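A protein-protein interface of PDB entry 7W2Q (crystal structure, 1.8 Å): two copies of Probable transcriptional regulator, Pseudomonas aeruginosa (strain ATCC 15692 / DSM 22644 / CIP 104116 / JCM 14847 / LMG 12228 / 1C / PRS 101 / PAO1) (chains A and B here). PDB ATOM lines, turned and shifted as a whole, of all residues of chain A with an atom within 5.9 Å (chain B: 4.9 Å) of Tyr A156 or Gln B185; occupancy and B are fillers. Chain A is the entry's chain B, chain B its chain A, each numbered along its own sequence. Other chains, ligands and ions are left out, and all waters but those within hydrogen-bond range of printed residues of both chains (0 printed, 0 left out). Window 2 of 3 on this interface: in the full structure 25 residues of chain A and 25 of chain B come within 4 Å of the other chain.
Val A153 touches none of the printed residues of chain B. Tyr A156 touches four residues of chain B. Of the printed residues of chain B, Cys A160 touches Trp B178 and Phe B188. Gln B185 touches one residue of chain A. Printed residues of chain A within 4 Å of Gly B187: Phe A157. The nearest printed residue of chain A that does not touch Val B181 is Cys A160 (6.3 Å).
Tyr A156 touches Trp B178 (CB to CH2, 3.9 Å). Tyr A156 touches Val B181 (CE1 to CG1, 3.98 Å). Leu B182 touches Tyr A156 (CD2 to CE1, 3.7 Å). Tyr A156 touches Gln B185 (OH to CD, 3.7 Å). C of Gly B187 touches CE2 of Phe A157 (3.9 Å). N of Phe B188 touches CZ of Phe A157 (3.6 Å). Trp B178 touches Tyr A159 (CZ2 to CD1, 3.7 Å). SG of Cys A160 touches CE3 of Trp B178, at 3.5 Å. Cys A160 touches Phe B188 (CB to CZ, 3.6 Å).
Printed residues of chain B that touch a printed residue of chain A: Trp B178, Val B181, Leu B182, Gln B185, Gly B187 and Phe B188. Among the printed residues, 9 pairs touch across the chains. Among the printed residues, no Asp or Glu carboxylate lies within 4 Å of a Lys or Arg side-chain nitrogen of the other chain.
SG of Cys A160 lies within hydrogen-bond range of O of Tyr A156, 3.3 Å away.
No position is printed for both chains. Of the 9 pairs that touch across the chains among the printed residues, none has its exchanged pair printed and touching as well.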
ATOM      1  N   ILE A 141      24.802  14.425 -15.424  1.00  0.00           N
ATOM      2  CA  ILE A 141      23.964  14.424 -16.620  1.00  0.00           C
ATOM      3  C   ILE A 141      24.746  13.884 -17.814  1.00  0.00           C
ATOM      4  O   ILE A 141      24.251  13.041 -18.567  1.00  0.00           O
ATOM      5  CB  ILE A 141      23.427  15.841 -16.896  1.00  0.00           C
ATOM      6  CG1 ILE A 141      22.313  16.209 -15.905  1.00  0.00           C
ATOM      7  CG2 ILE A 141      22.914  15.956 -18.325  1.00  0.00           C
ATOM      8  CD1 ILE A 141      22.023  17.698 -15.863  1.00  0.00           C
ATOM      9  N   VAL A 153      20.926  15.153 -25.849  1.00  0.00           N
ATOM     10  CA  VAL A 153      20.623  16.562 -26.087  1.00  0.00           C
ATOM     11  C   VAL A 153      21.639  17.358 -25.273  1.00  0.00           C
ATOM     12  O   VAL A 153      22.414  16.747 -24.522  1.00  0.00           O
ATOM     13  CB  VAL A 153      19.170  16.890 -25.702  1.00  0.00           C
ATOM     14  CG1 VAL A 153      18.200  16.046 -26.536  1.00  0.00           C
ATOM     15  CG2 VAL A 153      18.953  16.667 -24.220  1.00  0.00           C
ATOM     16  N   PRO A 154      21.718  18.685 -25.391  1.00  0.00           N
ATOM     17  CA  PRO A 154      22.687  19.428 -24.574  1.00  0.00           C
ATOM     18  C   PRO A 154      22.430  19.182 -23.103  1.00  0.00           C
ATOM     19  O   PRO A 154      21.267  19.102 -22.679  1.00  0.00           O
ATOM     20  CB  PRO A 154      22.429  20.899 -24.952  1.00  0.00           C
ATOM     21  CG  PRO A 154      21.877  20.820 -26.329  1.00  0.00           C
ATOM     22  CD  PRO A 154      21.011  19.578 -26.326  1.00  0.00           C
ATOM     23  N   PRO A 155      23.477  19.016 -22.301  1.00  0.00           N
ATOM     24  CA  PRO A 155      23.261  18.798 -20.860  1.00  0.00           C
ATOM     25  C   PRO A 155      22.396  19.846 -20.191  1.00  0.00           C
ATOM     26  O   PRO A 155      21.633  19.508 -19.275  1.00  0.00           O
ATOM     27  CB  PRO A 155      24.685  18.789 -20.310  1.00  0.00           C
ATOM     28  CG  PRO A 155      25.466  18.170 -21.427  1.00  0.00           C
ATOM     29  CD  PRO A 155      24.880  18.779 -22.680  1.00  0.00           C
ATOM     30  N   TYR A 156      22.464  21.111 -20.621  1.00  0.00           N
ATOM     31  CA  TYR A 156      21.633  22.120 -19.973  1.00  0.00           C
ATOM     32  C   TYR A 156      20.147  21.893 -20.227  1.00  0.00           C
ATOM     33  O   TYR A 156      19.336  22.388 -19.452  1.00  0.00           O
ATOM     34  CB  TYR A 156      22.048  23.518 -20.400  1.00  0.00           C
ATOM     35  CG  TYR A 156      21.575  23.990 -21.752  1.00  0.00           C
ATOM     36  CD1 TYR A 156      20.341  24.626 -21.906  1.00  0.00           C
ATOM     37  CD2 TYR A 156      22.392  23.862 -22.867  1.00  0.00           C
ATOM     38  CE1 TYR A 156      19.925  25.088 -23.144  1.00  0.00           C
ATOM     39  CE2 TYR A 156      21.986  24.329 -24.111  1.00  0.00           C
ATOM     40  CZ  TYR A 156      20.762  24.948 -24.241  1.00  0.00           C
ATOM     41  OH  TYR A 156      20.359  25.398 -25.478  1.00  0.00           O
ATOM     42  N   PHE A 157      19.771  21.148 -21.276  1.00  0.00           N
ATOM     43  CA  PHE A 157      18.371  20.757 -21.427  1.00  0.00           C
ATOM     44  C   PHE A 157      17.905  19.998 -20.196  1.00  0.00           C
ATOM     45  O   PHE A 157      16.875  20.331 -19.591  1.00  0.00           O
ATOM     46  CB  PHE A 157      18.177  19.876 -22.667  1.00  0.00           C
ATOM     47  CG  PHE A 157      18.068  20.634 -23.968  1.00  0.00           C
ATOM     48  CD1 PHE A 157      18.728  21.828 -24.159  1.00  0.00           C
ATOM     49  CD2 PHE A 157      17.306  20.119 -25.007  1.00  0.00           C
ATOM     50  CE1 PHE A 157      18.630  22.507 -25.370  1.00  0.00           C
ATOM     51  CE2 PHE A 157      17.199  20.784 -26.211  1.00  0.00           C
ATOM     52  CZ  PHE A 157      17.864  21.985 -26.392  1.00  0.00           C
ATOM     53  N   HIS A 158      18.664  18.967 -19.816  1.00  0.00           N
ATOM     54  CA  HIS A 158      18.349  18.171 -18.639  1.00  0.00           C
ATOM     55  C   HIS A 158      18.470  18.989 -17.363  1.00  0.00           C
ATOM     56  O   HIS A 158      17.648  18.848 -16.456  1.00  0.00           O
ATOM     57  CB  HIS A 158      19.271  16.955 -18.574  1.00  0.00           C
ATOM     58  CG  HIS A 158      19.102  16.015 -19.720  1.00  0.00           C
ATOM     59  ND1 HIS A 158      17.985  15.222 -19.873  1.00  0.00           N
ATOM     60  CD2 HIS A 158      19.916  15.731 -20.772  1.00  0.00           C
ATOM     61  CE1 HIS A 158      18.116  14.486 -20.964  1.00  0.00           C
ATOM     62  NE2 HIS A 158      19.276  14.777 -21.527  1.00  0.00           N
ATOM     63  N   TYR A 159      19.513  19.819 -17.255  1.00  0.00           N
ATOM     64  CA  TYR A 159      19.666  20.640 -16.057  1.00  0.00           C
ATOM     65  C   TYR A 159      18.449  21.527 -15.851  1.00  0.00           C
ATOM     66  O   TYR A 159      17.941  21.663 -14.727  1.00  0.00           O
ATOM     67  CB  TYR A 159      20.933  21.495 -16.162  1.00  0.00           C
ATOM     68  CG  TYR A 159      21.172  22.341 -14.930  1.00  0.00           C
ATOM     69  CD1 TYR A 159      20.593  23.600 -14.798  1.00  0.00           C
ATOM     70  CD2 TYR A 159      21.953  21.866 -13.887  1.00  0.00           C
ATOM     71  CE1 TYR A 159      20.798  24.376 -13.665  1.00  0.00           C
ATOM     72  CE2 TYR A 159      22.166  22.634 -12.749  1.00  0.00           C
ATOM     73  CZ  TYR A 159      21.587  23.880 -12.647  1.00  0.00           C
ATOM     74  OH  TYR A 159      21.792  24.624 -11.523  1.00  0.00           O
ATOM     75  N   CYS A 160      17.991  22.185 -16.922  1.00  0.00           N
ATOM     76  CA  CYS A 160      16.887  23.132 -16.782  1.00  0.00           C
ATOM     77  C   CYS A 160      15.580  22.411 -16.492  1.00  0.00           C
ATOM     78  O   CYS A 160      14.743  22.924 -15.740  1.00  0.00           O
ATOM     79  CB  CYS A 160      16.762  23.993 -18.037  1.00  0.00           C
ATOM     80  SG  CYS A 160      18.070  25.219 -18.216  1.00  0.00           S
ATOM     81  N   ALA A 161      15.387  21.221 -17.076  1.00  0.00           N
ATOM     82  CA  ALA A 161      14.190  20.447 -16.747  1.00  0.00           C
ATOM     83  C   ALA A 161      14.169  20.081 -15.266  1.00  0.00           C
ATOM     84  O   ALA A 161      13.125  20.177 -14.608  1.00  0.00           O
ATOM     85  CB  ALA A 161      14.117  19.197 -17.617  1.00  0.00           C
ATOM     86  N   TRP B 178      18.986  32.226 -17.318  1.00  0.00           N
ATOM     87  CA  TRP B 178      18.532  31.255 -18.306  1.00  0.00           C
ATOM     88  C   TRP B 178      17.688  31.869 -19.416  1.00  0.00           C
ATOM     89  O   TRP B 178      17.635  31.307 -20.514  1.00  0.00           O
ATOM     90  CB  TRP B 178      17.760  30.130 -17.612  1.00  0.00           C
ATOM     91  CG  TRP B 178      18.664  29.212 -16.863  1.00  0.00           C
ATOM     92  CD1 TRP B 178      18.724  29.034 -15.512  1.00  0.00           C
ATOM     93  CD2 TRP B 178      19.654  28.343 -17.429  1.00  0.00           C
ATOM     94  NE1 TRP B 178      19.699  28.109 -15.202  1.00  0.00           N
ATOM     95  CE2 TRP B 178      20.277  27.666 -16.363  1.00  0.00           C
ATOM     96  CE3 TRP B 178      20.074  28.080 -18.732  1.00  0.00           C
ATOM     97  CZ2 TRP B 178      21.301  26.738 -16.560  1.00  0.00           C
ATOM     98  CZ3 TRP B 178      21.092  27.144 -18.934  1.00  0.00           C
ATOM     99  CH2 TRP B 178      21.691  26.488 -17.851  1.00  0.00           C
ATOM    100  N   VAL B 181      19.517  32.463 -22.519  1.00  0.00           N
ATOM    101  CA  VAL B 181      19.973  31.196 -23.087  1.00  0.00           C
ATOM    102  C   VAL B 181      18.846  30.504 -23.841  1.00  0.00           C
ATOM    103  O   VAL B 181      19.058  29.911 -24.910  1.00  0.00           O
ATOM    104  CB  VAL B 181      20.525  30.291 -21.970  1.00  0.00           C
ATOM    105  CG1 VAL B 181      20.880  28.901 -22.529  1.00  0.00           C
ATOM    106  CG2 VAL B 181      21.732  30.940 -21.301  1.00  0.00           C
ATOM    107  N   LEU B 182      17.634  30.550 -23.289  1.00  0.00           N
ATOM    108  CA  LEU B 182      16.538  29.710 -23.755  1.00  0.00           C
ATOM    109  C   LEU B 182      15.602  30.388 -24.745  1.00  0.00           C
ATOM    110  O   LEU B 182      14.850  29.689 -25.429  1.00  0.00           O
ATOM    111  CB  LEU B 182      15.710  29.225 -22.559  1.00  0.00           C
ATOM    112  CG  LEU B 182      16.465  28.447 -21.488  1.00  0.00           C
ATOM    113  CD1 LEU B 182      15.561  28.196 -20.274  1.00  0.00           C
ATOM    114  CD2 LEU B 182      17.005  27.131 -22.052  1.00  0.00           C
ATOM    115  N   GLU B 183      15.614  31.723 -24.832  1.00  0.00           N
ATOM    116  CA  GLU B 183      14.532  32.435 -25.512  1.00  0.00           C
ATOM    117  C   GLU B 183      14.397  32.029 -26.978  1.00  0.00           C
ATOM    118  O   GLU B 183      13.279  31.993 -27.508  1.00  0.00           O
ATOM    119  CB  GLU B 183      14.734  33.952 -25.381  1.00  0.00           C
ATOM    120  CG  GLU B 183      15.903  34.523 -26.179  1.00  0.00           C
ATOM    121  CD  GLU B 183      16.071  36.018 -25.973  1.00  0.00           C
ATOM    122  OE1 GLU B 183      17.073  36.581 -26.464  1.00  0.00           O
ATOM    123  OE2 GLU B 183      15.203  36.630 -25.312  1.00  0.00           O
ATOM    124  N   ASP B 184      15.507  31.706 -27.640  1.00  0.00           N
ATOM    125  CA  ASP B 184      15.513  31.343 -29.050  1.00  0.00           C
ATOM    126  C   ASP B 184      15.543  29.836 -29.298  1.00  0.00           C
ATOM    127  O   ASP B 184      15.614  29.418 -30.458  1.00  0.00           O
ATOM    128  CB  ASP B 184      16.720  31.987 -29.730  1.00  0.00           C
ATOM    129  CG  ASP B 184      17.963  31.930 -28.863  1.00  0.00           C
ATOM    130  OD1 ASP B 184      17.822  31.605 -27.660  1.00  0.00           O
ATOM    131  OD2 ASP B 184      19.069  32.205 -29.377  1.00  0.00           O
ATOM    132  N   GLN B 185      15.487  29.010 -28.256  1.00  0.00           N
ATOM    133  CA  GLN B 185      15.728  27.570 -28.387  1.00  0.00           C
ATOM    134  C   GLN B 185      14.391  26.840 -28.500  1.00  0.00           C
ATOM    135  O   GLN B 185      13.805  26.413 -27.498  1.00  0.00           O
ATOM    136  CB  GLN B 185      16.552  27.063 -27.207  1.00  0.00           C
ATOM    137  CG  GLN B 185      17.930  27.716 -27.101  1.00  0.00           C
ATOM    138  CD  GLN B 185      18.845  27.334 -28.245  1.00  0.00           C
ATOM    139  OE1 GLN B 185      18.719  26.255 -28.824  1.00  0.00           O
ATOM    140  NE2 GLN B 185      19.773  28.221 -28.579  1.00  0.00           N
ATOM    141  N   GLU B 186      13.901  26.711 -29.738  1.00  0.00           N
ATOM    142  CA  GLU B 186      12.648  25.998 -29.970  1.00  0.00           C
ATOM    143  C   GLU B 186      12.779  24.521 -29.624  1.00  0.00           C
ATOM    144  O   GLU B 186      11.805  23.901 -29.182  1.00  0.00           O
ATOM    145  CB  GLU B 186      12.205  26.163 -31.426  1.00  0.00           C
ATOM    146  CG  GLU B 186      11.198  27.266 -31.672  1.00  0.00           C
ATOM    147  CD  GLU B 186       9.940  27.117 -30.828  1.00  0.00           C
ATOM    148  OE1 GLU B 186       9.880  27.725 -29.739  1.00  0.00           O
ATOM    149  OE2 GLU B 186       9.011  26.400 -31.258  1.00  0.00           O
ATOM    150  N   GLY B 187      13.969  23.948 -29.815  1.00  0.00           N
ATOM    151  CA  GLY B 187      14.183  22.553 -29.451  1.00  0.00           C
ATOM    152  C   GLY B 187      14.070  22.311 -27.959  1.00  0.00           C
ATOM    153  O   GLY B 187      13.528  21.285 -27.528  1.00  0.00           O
ATOM    154  N   PHE B 188      14.584  23.246 -27.145  1.00  0.00           N
ATOM    155  CA  PHE B 188      14.418  23.108 -25.701  1.00  0.00           C
ATOM    156  C   PHE B 188      12.951  23.199 -25.308  1.00  0.00           C
ATOM    157  O   PHE B 188      12.488  22.453 -24.436  1.00  0.00           O
ATOM    158  CB  PHE B 188      15.208  24.167 -24.926  1.00  0.00           C
ATOM    159  CG  PHE B 188      14.930  24.118 -23.454  1.00  0.00           C
ATOM    160  CD1 PHE B 188      15.448  23.082 -22.682  1.00  0.00           C
ATOM    161  CD2 PHE B 188      14.076  25.041 -22.857  1.00  0.00           C
ATOM    162  CE1 PHE B 188      15.176  23.002 -21.327  1.00  0.00           C
ATOM    163  CE2 PHE B 188      13.792  24.964 -21.508  1.00  0.00           C
ATOM    164  CZ  PHE B 188      14.329  23.943 -20.743  1.00  0.00           C
ATOM    165  N   PHE B 189      12.208  24.111 -25.933  1.00  0.00           N
ATOM    166  CA  PHE B 189      10.785  24.216 -25.633  1.00  0.00           C
ATOM    167  C   PHE B 189      10.068  22.916 -25.964  1.00  0.00           C
ATOM    168  O   PHE B 189       9.239  22.435 -25.183  1.00  0.00           O
ATOM    169  CB  PHE B 189      10.161  25.375 -26.397  1.00  0.00           C
ATOM    170  CG  PHE B 189       8.734  25.648 -25.998  1.00  0.00           C
ATOM    171  CD1 PHE B 189       8.448  26.430 -24.895  1.00  0.00           C
ATOM    172  CD2 PHE B 189       7.683  25.102 -26.716  1.00  0.00           C
ATOM    173  CE1 PHE B 189       7.135  26.667 -24.523  1.00  0.00           C
ATOM    174  CE2 PHE B 189       6.378  25.340 -26.354  1.00  0.00           C
ATOM    175  CZ  PHE B 189       6.106  26.120 -25.253  1.00  0.00           C
